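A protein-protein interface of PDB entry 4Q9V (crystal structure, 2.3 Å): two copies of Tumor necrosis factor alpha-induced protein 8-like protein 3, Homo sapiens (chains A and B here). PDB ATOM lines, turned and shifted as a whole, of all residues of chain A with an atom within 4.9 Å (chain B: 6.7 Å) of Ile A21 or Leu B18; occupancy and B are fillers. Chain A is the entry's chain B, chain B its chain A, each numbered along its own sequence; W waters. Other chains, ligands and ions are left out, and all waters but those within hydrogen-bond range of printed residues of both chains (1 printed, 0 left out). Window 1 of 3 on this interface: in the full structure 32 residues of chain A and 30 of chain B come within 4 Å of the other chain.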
ATOM      1  N   ILE A  17      13.823 -13.373  13.016  1.00  0.00           N
ATOM      2  CA  ILE A  17      13.422 -14.414  13.979  1.00  0.00           C
ATOM      3  C   ILE A  17      11.995 -14.221  14.485  1.00  0.00           C
ATOM      4  O   ILE A  17      11.220 -15.190  14.587  1.00  0.00           O
ATOM      5  CB  ILE A  17      14.395 -14.503  15.179  1.00  0.00           C
ATOM      6  CG1 ILE A  17      15.691 -15.196  14.756  1.00  0.00           C
ATOM      7  CG2 ILE A  17      13.768 -15.268  16.339  1.00  0.00           C
ATOM      8  CD1 ILE A  17      16.877 -14.870  15.663  1.00  0.00           C
ATOM      9  N   LEU A  18      11.646 -12.971  14.772  1.00  0.00           N
ATOM     10  CA  LEU A  18      10.325 -12.645  15.286  1.00  0.00           C
ATOM     11  C   LEU A  18       9.261 -12.777  14.192  1.00  0.00           C
ATOM     12  O   LEU A  18       8.119 -13.203  14.478  1.00  0.00           O
ATOM     13  CB  LEU A  18      10.293 -11.248  15.925  1.00  0.00           C
ATOM     14  CG  LEU A  18      11.019 -10.993  17.257  1.00  0.00           C
ATOM     15  CD1 LEU A  18      10.780  -9.583  17.735  1.00  0.00           C
ATOM     16  CD2 LEU A  18      10.606 -11.949  18.346  1.00  0.00           C
ATOM     17  N   SER A  19       9.613 -12.431  12.949  1.00  0.00           N
ATOM     18  CA  SER A  19       8.639 -12.659  11.875  1.00  0.00           C
ATOM     19  C   SER A  19       8.362 -14.166  11.692  1.00  0.00           C
ATOM     20  O   SER A  19       7.204 -14.601  11.688  1.00  0.00           O
ATOM     21  CB  SER A  19       9.057 -11.983  10.565  1.00  0.00           C
ATOM     22  OG  SER A  19      10.050 -12.723   9.892  1.00  0.00           O
ATOM     23  N   LYS A  20       9.427 -14.949  11.578  1.00  0.00           N
ATOM     24  CA  LYS A  20       9.305 -16.396  11.464  1.00  0.00           C
ATOM     25  C   LYS A  20       8.431 -16.967  12.578  1.00  0.00           C
ATOM     26  O   LYS A  20       7.595 -17.836  12.338  1.00  0.00           O
ATOM     27  CB  LYS A  20      10.685 -17.055  11.489  1.00  0.00           C
ATOM     28  CG  LYS A  20      11.058 -17.761  10.197  1.00  0.00           C
ATOM     29  CD  LYS A  20      12.465 -17.397   9.750  1.00  0.00           C
ATOM     30  CE  LYS A  20      12.960 -18.342   8.666  1.00  0.00           C
ATOM     31  NZ  LYS A  20      14.046 -17.738   7.845  1.00  0.00           N
ATOM     32  N   ILE A  21       8.626 -16.476  13.797  1.00  0.00           N
ATOM     33  CA  ILE A  21       7.831 -16.928  14.934  1.00  0.00           C
ATOM     34  C   ILE A  21       6.354 -16.630  14.695  1.00  0.00           C
ATOM     35  O   ILE A  21       5.500 -17.486  14.910  1.00  0.00           O
ATOM     36  CB  ILE A  21       8.306 -16.286  16.254  1.00  0.00           C
ATOM     37  CG1 ILE A  21       9.681 -16.828  16.641  1.00  0.00           C
ATOM     38  CG2 ILE A  21       7.315 -16.545  17.380  1.00  0.00           C
ATOM     39  CD1 ILE A  21      10.087 -16.502  18.059  1.00  0.00           C
ATOM     40  N   ALA A  22       6.061 -15.416  14.247  1.00  0.00           N
ATOM     41  CA  ALA A  22       4.688 -15.043  13.939  1.00  0.00           C
ATOM     42  C   ALA A  22       4.086 -16.050  12.967  1.00  0.00           C
ATOM     43  O   ALA A  22       2.960 -16.508  13.150  1.00  0.00           O
ATOM     44  CB  ALA A  22       4.635 -13.640  13.358  1.00  0.00           C
ATOM     45  N   SER A  23       4.849 -16.399  11.938  1.00  0.00           N
ATOM     46  CA  SER A  23       4.404 -17.369  10.947  1.00  0.00           C
ATOM     47  C   SER A  23       4.128 -18.720  11.592  1.00  0.00           C
ATOM     48  O   SER A  23       2.983 -19.160  11.668  1.00  0.00           O
ATOM     49  CB  SER A  23       5.453 -17.528   9.848  1.00  0.00           C
ATOM     50  OG  SER A  23       5.543 -16.360   9.052  1.00  0.00           O
ATOM     51  N   LYS A  24       5.188 -19.372  12.056  1.00  0.00           N
ATOM     52  CA  LYS A  24       5.076 -20.681  12.685  1.00  0.00           C
ATOM     53  C   LYS A  24       3.899 -20.745  13.651  1.00  0.00           C
ATOM     54  O   LYS A  24       3.168 -21.735  13.685  1.00  0.00           O
ATOM     55  CB  LYS A  24       6.371 -21.037  13.416  1.00  0.00           C
ATOM     56  CG  LYS A  24       7.411 -21.715  12.539  1.00  0.00           C
ATOM     57  CD  LYS A  24       7.318 -23.228  12.641  1.00  0.00           C
ATOM     58  CE  LYS A  24       8.304 -23.905  11.704  1.00  0.00           C
ATOM     59  NZ  LYS A  24       9.597 -24.209  12.381  1.00  0.00           N
ATOM     60  N   THR A  25       3.719 -19.689  14.435  1.00  0.00           N
ATOM     61  CA  THR A  25       2.633 -19.647  15.408  1.00  0.00           C
ATOM     62  C   THR A  25       1.281 -19.704  14.713  1.00  0.00           C
ATOM     63  O   THR A  25       0.395 -20.446  15.133  1.00  0.00           O
ATOM     64  CB  THR A  25       2.711 -18.394  16.298  1.00  0.00           C
ATOM     65  OG1 THR A  25       3.878 -18.469  17.126  1.00  0.00           O
ATOM     66  CG2 THR A  25       1.480 -18.290  17.186  1.00  0.00           C
ATOM     67  N   VAL A  26       1.120 -18.922  13.652  1.00  0.00           N
ATOM     68  CA  VAL A  26      -0.134 -18.959  12.886  1.00  0.00           C
ATOM     69  C   VAL A  26      -0.394 -20.356  12.282  1.00  0.00           C
ATOM     70  O   VAL A  26      -1.540 -20.824  12.237  1.00  0.00           O
ATOM     71  CB  VAL A  26      -0.196 -17.856  11.797  1.00  0.00           C
ATOM     72  CG1 VAL A  26      -1.486 -17.963  10.992  1.00  0.00           C
ATOM     73  CG2 VAL A  26      -0.072 -16.474  12.436  1.00  0.00           C
ATOM     74  N   ILE A  72       3.703 -24.444  25.668  1.00  0.00           N
ATOM     75  CA  ILE A  72       5.051 -24.037  25.290  1.00  0.00           C
ATOM     76  C   ILE A  72       6.109 -24.836  26.063  1.00  0.00           C
ATOM     77  O   ILE A  72       7.059 -25.350  25.453  1.00  0.00           O
ATOM     78  CB  ILE A  72       5.242 -22.507  25.420  1.00  0.00           C
ATOM     79  CG1 ILE A  72       4.633 -21.816  24.197  1.00  0.00           C
ATOM     80  CG2 ILE A  72       6.724 -22.157  25.507  1.00  0.00           C
ATOM     81  CD1 ILE A  72       4.341 -20.342  24.397  1.00  0.00           C
ATOM     82  N   ASN A  76       8.638 -27.192  24.060  1.00  0.00           N
ATOM     83  CA  ASN A  76      10.072 -26.943  24.235  1.00  0.00           C
ATOM     84  C   ASN A  76      10.787 -27.851  25.222  1.00  0.00           C
ATOM     85  O   ASN A  76      11.845 -27.478  25.748  1.00  0.00           O
ATOM     86  CB  ASN A  76      10.305 -25.488  24.652  1.00  0.00           C
ATOM     87  CG  ASN A  76      10.111 -24.537  23.512  1.00  0.00           C
ATOM     88  OD1 ASN A  76      10.083 -24.950  22.347  1.00  0.00           O
ATOM     89  ND2 ASN A  76       9.962 -23.255  23.825  1.00  0.00           N
ATOM     90  N   ALA B  13      -1.137 -14.366  22.554  1.00  0.00           N
ATOM     91  CA  ALA B  13      -0.398 -14.884  23.705  1.00  0.00           C
ATOM     92  C   ALA B  13       0.760 -15.804  23.301  1.00  0.00           C
ATOM     93  O   ALA B  13       1.874 -15.695  23.832  1.00  0.00           O
ATOM     94  CB  ALA B  13      -1.343 -15.587  24.659  1.00  0.00           C
ATOM     95  N   GLN B  14       0.510 -16.684  22.339  1.00  0.00           N
ATOM     96  CA  GLN B  14       1.552 -17.607  21.895  1.00  0.00           C
ATOM     97  C   GLN B  14       2.696 -16.875  21.197  1.00  0.00           C
ATOM     98  O   GLN B  14       3.889 -17.165  21.445  1.00  0.00           O
ATOM     99  CB  GLN B  14       0.966 -18.664  20.962  1.00  0.00           C
ATOM    100  CG  GLN B  14       1.978 -19.690  20.452  1.00  0.00           C
ATOM    101  CD  GLN B  14       1.309 -20.879  19.755  1.00  0.00           C
ATOM    102  OE1 GLN B  14       0.149 -21.208  20.025  1.00  0.00           O
ATOM    103  NE2 GLN B  14       2.044 -21.525  18.863  1.00  0.00           N
ATOM    104  N   LYS B  15       2.328 -15.947  20.309  1.00  0.00           N
ATOM    105  CA  LYS B  15       3.320 -15.128  19.619  1.00  0.00           C
ATOM    106  C   LYS B  15       4.196 -14.407  20.640  1.00  0.00           C
ATOM    107  O   LYS B  15       5.412 -14.466  20.569  1.00  0.00           O
ATOM    108  CB  LYS B  15       2.631 -14.099  18.714  1.00  0.00           C
ATOM    109  CG  LYS B  15       2.084 -14.654  17.400  1.00  0.00           C
ATOM    110  CD  LYS B  15       1.326 -13.571  16.614  1.00  0.00           C
ATOM    111  CE  LYS B  15       0.882 -14.100  15.258  1.00  0.00           C
ATOM    112  NZ  LYS B  15       0.053 -13.134  14.492  1.00  0.00           N
ATOM    113  N   LYS B  16       3.546 -13.760  21.601  1.00  0.00           N
ATOM    114  CA  LYS B  16       4.195 -12.977  22.640  1.00  0.00           C
ATOM    115  C   LYS B  16       5.156 -13.774  23.492  1.00  0.00           C
ATOM    116  O   LYS B  16       6.293 -13.352  23.687  1.00  0.00           O
ATOM    117  CB  LYS B  16       3.142 -12.315  23.536  1.00  0.00           C
ATOM    118  CG  LYS B  16       3.716 -11.631  24.758  1.00  0.00           C
ATOM    119  CD  LYS B  16       2.801 -10.514  25.257  1.00  0.00           C
ATOM    120  CE  LYS B  16       3.470  -9.708  26.371  1.00  0.00           C
ATOM    121  NZ  LYS B  16       3.016  -8.278  26.423  1.00  0.00           N
ATOM    122  N   ILE B  17       4.716 -14.913  24.012  1.00  0.00           N
ATOM    123  CA  ILE B  17       5.617 -15.705  24.858  1.00  0.00           C
ATOM    124  C   ILE B  17       6.793 -16.219  24.034  1.00  0.00           C
ATOM    125  O   ILE B  17       7.966 -16.197  24.486  1.00  0.00           O
ATOM    126  CB  ILE B  17       4.882 -16.891  25.553  1.00  0.00           C
ATOM    127  CG1 ILE B  17       3.722 -16.376  26.407  1.00  0.00           C
ATOM    128  CG2 ILE B  17       5.849 -17.713  26.407  1.00  0.00           C
ATOM    129  CD1 ILE B  17       4.078 -15.125  27.237  1.00  0.00           C
ATOM    130  N   LEU B  18       6.487 -16.670  22.819  1.00  0.00           N
ATOM    131  CA  LEU B  18       7.557 -17.185  21.966  1.00  0.00           C
ATOM    132  C   LEU B  18       8.603 -16.087  21.656  1.00  0.00           C
ATOM    133  O   LEU B  18       9.817 -16.321  21.682  1.00  0.00           O
ATOM    134  CB  LEU B  18       6.960 -17.793  20.687  1.00  0.00           C
ATOM    135  CG  LEU B  18       6.874 -19.325  20.589  1.00  0.00           C
ATOM    136  CD1 LEU B  18       6.980 -19.990  21.947  1.00  0.00           C
ATOM    137  CD2 LEU B  18       5.601 -19.768  19.888  1.00  0.00           C
ATOM    138  N   SER B  19       8.103 -14.881  21.410  1.00  0.00           N
ATOM    139  CA  SER B  19       8.907 -13.725  21.022  1.00  0.00           C
ATOM    140  C   SER B  19       9.769 -13.252  22.169  1.00  0.00           C
ATOM    141  O   SER B  19      10.971 -12.992  22.004  1.00  0.00           O
ATOM    142  CB  SER B  19       7.992 -12.586  20.566  1.00  0.00           C
ATOM    143  OG  SER B  19       7.420 -12.900  19.310  1.00  0.00           O
ATOM    144  N   LYS B  20       9.139 -13.143  23.335  1.00  0.00           N
ATOM    145  CA  LYS B  20       9.836 -12.802  24.559  1.00  0.00           C
ATOM    146  C   LYS B  20      10.992 -13.766  24.801  1.00  0.00           C
ATOM    147  O   LYS B  20      12.132 -13.333  25.045  1.00  0.00           O
ATOM    148  CB  LYS B  20       8.870 -12.806  25.746  1.00  0.00           C
ATOM    149  CG  LYS B  20       9.606 -12.831  27.088  1.00  0.00           C
ATOM    150  CD  LYS B  20       8.788 -12.212  28.220  1.00  0.00           C
ATOM    151  CE  LYS B  20       9.672 -11.946  29.439  1.00  0.00           C
ATOM    152  NZ  LYS B  20       9.004 -11.058  30.431  1.00  0.00           N
ATOM    153  N   ILE B  21      10.711 -15.066  24.698  1.00  0.00           N
ATOM    154  CA  ILE B  21      11.792 -16.053  24.795  1.00  0.00           C
ATOM    155  C   ILE B  21      12.914 -15.785  23.790  1.00  0.00           C
ATOM    156  O   ILE B  21      14.114 -15.766  24.158  1.00  0.00           O
ATOM    157  CB  ILE B  21      11.285 -17.504  24.595  1.00  0.00           C
ATOM    158  CG1 ILE B  21      10.311 -17.895  25.704  1.00  0.00           C
ATOM    159  CG2 ILE B  21      12.461 -18.491  24.557  1.00  0.00           C
ATOM    160  CD1 ILE B  21       9.758 -19.336  25.549  1.00  0.00           C
ATOM    161  N   ALA B  22      12.535 -15.582  22.527  1.00  0.00           N
ATOM    162  CA  ALA B  22      13.544 -15.363  21.466  1.00  0.00           C
ATOM    163  C   ALA B  22      14.486 -14.157  21.736  1.00  0.00           C
ATOM    164  O   ALA B  22      15.732 -14.226  21.621  1.00  0.00           O
ATOM    165  CB  ALA B  22      12.834 -15.195  20.127  1.00  0.00           C
ATOM    166  N   SER B  23      13.869 -13.043  22.103  1.00  0.00           N
ATOM    167  CA  SER B  23      14.603 -11.809  22.303  1.00  0.00           C
ATOM    168  C   SER B  23      15.427 -11.868  23.576  1.00  0.00           C
ATOM    169  O   SER B  23      16.524 -11.317  23.620  1.00  0.00           O
ATOM    170  CB  SER B  23      13.649 -10.624  22.317  1.00  0.00           C
ATOM    171  OG  SER B  23      12.788 -10.716  23.416  1.00  0.00           O
ATOM    172  N   ASN B  76      15.727 -23.488  23.844  1.00  0.00           N
ATOM    173  CA  ASN B  76      14.478 -24.168  23.545  1.00  0.00           C
ATOM    174  C   ASN B  76      14.562 -25.682  23.740  1.00  0.00           C
ATOM    175  O   ASN B  76      13.626 -26.385  23.404  1.00  0.00           O
ATOM    176  CB  ASN B  76      14.011 -23.853  22.116  1.00  0.00           C
ATOM    177  CG  ASN B  76      13.465 -22.440  21.974  1.00  0.00           C
ATOM    178  OD1 ASN B  76      13.446 -21.661  22.932  1.00  0.00           O
ATOM    179  ND2 ASN B  76      13.032 -22.099  20.766  1.00  0.00           N
HETATM  180  O   HOH W   1       6.540 -12.304  17.007  1.00  0.00           O
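Of the 12 printed residues of chain A, 8 touch a printed residue of chain B.
Hydrophobic or aromatic side chains of chain A within 4 Å of the printed part of chain B: Ile A17, Leu A18, Ile A21, Val A26 and Ile A72.
Printed residues of chain B that touch a printed residue of chain A: Gln B14, Lys B15, Ile B17, Leu B18, Ser B19, Ala B22 and Asn B76.
Hydrophobic or aromatic side chains of chain B that line the printed part of chain A: Ile B17, Leu B18 and Ala B22.
Among the printed residues, no Asp or Glu carboxylate lies within 4 Å of a Lys or Arg side-chain nitrogen of the other chain.
Water W1 bridges the side-chain hydroxyl (OG) of Ser B19 and the backbone carbonyl oxygen (O) of Leu A18.
Printed residues of chain B within 4 Å of Ile A17: Ala B22.
Printed residues of chain B within 4 Å of Leu A18: Ser B19 (3.5 Å).
Of chain B, only Leu B18 and Ala B22 come within 4 Å of Ile A21.
Of the printed residues of chain B, Ile A72 touches Ile B17 and Leu B18.
Of chain A, only Ile A21, Thr A25 and Ile A72 come within 4 Å of Leu B18.
The nearest residue of chain B that does not touch Ile A21 is Ser B19 (4.1 Å).
The nearest residue of chain A that does not touch Leu B18 is Asn A76 (4.8 Å).
The nearest printed residue of chain A that does not touch Asn B76 is Ile A21 (6.9 Å).
O of Asn A76 sits close to O of Asn B76.
Leu A18 touches Ser B19.
CB of Leu B18 touches CG2 of Ile A21, at 3.6 Å.
Ile A21 touches Ala B22 (CD1 to CB, 3.7 Å).
Ala A22 touches Lys B15.
Gln B14 touches Thr A25 (CG to CG2, 3.6 Å).
CG2 of Thr A25 touches CG of Lys B15, 3.7 Å away.
CD2 of Leu B18 touches OG1 of Thr A25 (3.5 Å).
Lys B15 touches Val A26.
CG2 of Ile B17 touches CD1 of Ile A72 (3.6 Å).
CD1 of Leu B18 touches CD1 of Ile A72, 3.6 Å away.
The side-chain hydroxyl (OG) of Ser B19 lies within hydrogen-bond range of the backbone carbonyl oxygen (O) of Lys B15.
The backbone carbonyl oxygen (O) of Ser B19 is in hydrogen-bond range of the side-chain hydroxyl (OG) of Ser B23 (3.2 Å).
The side-chain hydroxyl (OG1) of Thr A25 lies within hydrogen-bond range of the backbone carbonyl oxygen (O) of Ile A21, 2.9 Å away.
Leu A18 touches Ser B19, but with the chains exchanged Ser A19 does not touch Leu B18 (9.5 Å).
Ile A21 touches Leu B18, but with the chains exchanged Leu A18 does not touch Ile B21 (7.0 Å).
Ile A21 touches Ala B22, but with the chains exchanged Ala A22 does not touch Ile B21 (11.4 Å).
Asn B76 touches its own counterpart, Asn A76.
Of the 12 pairs that touch across the chains among the printed residues, 1 has its exchanged pair printed and touching as well.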
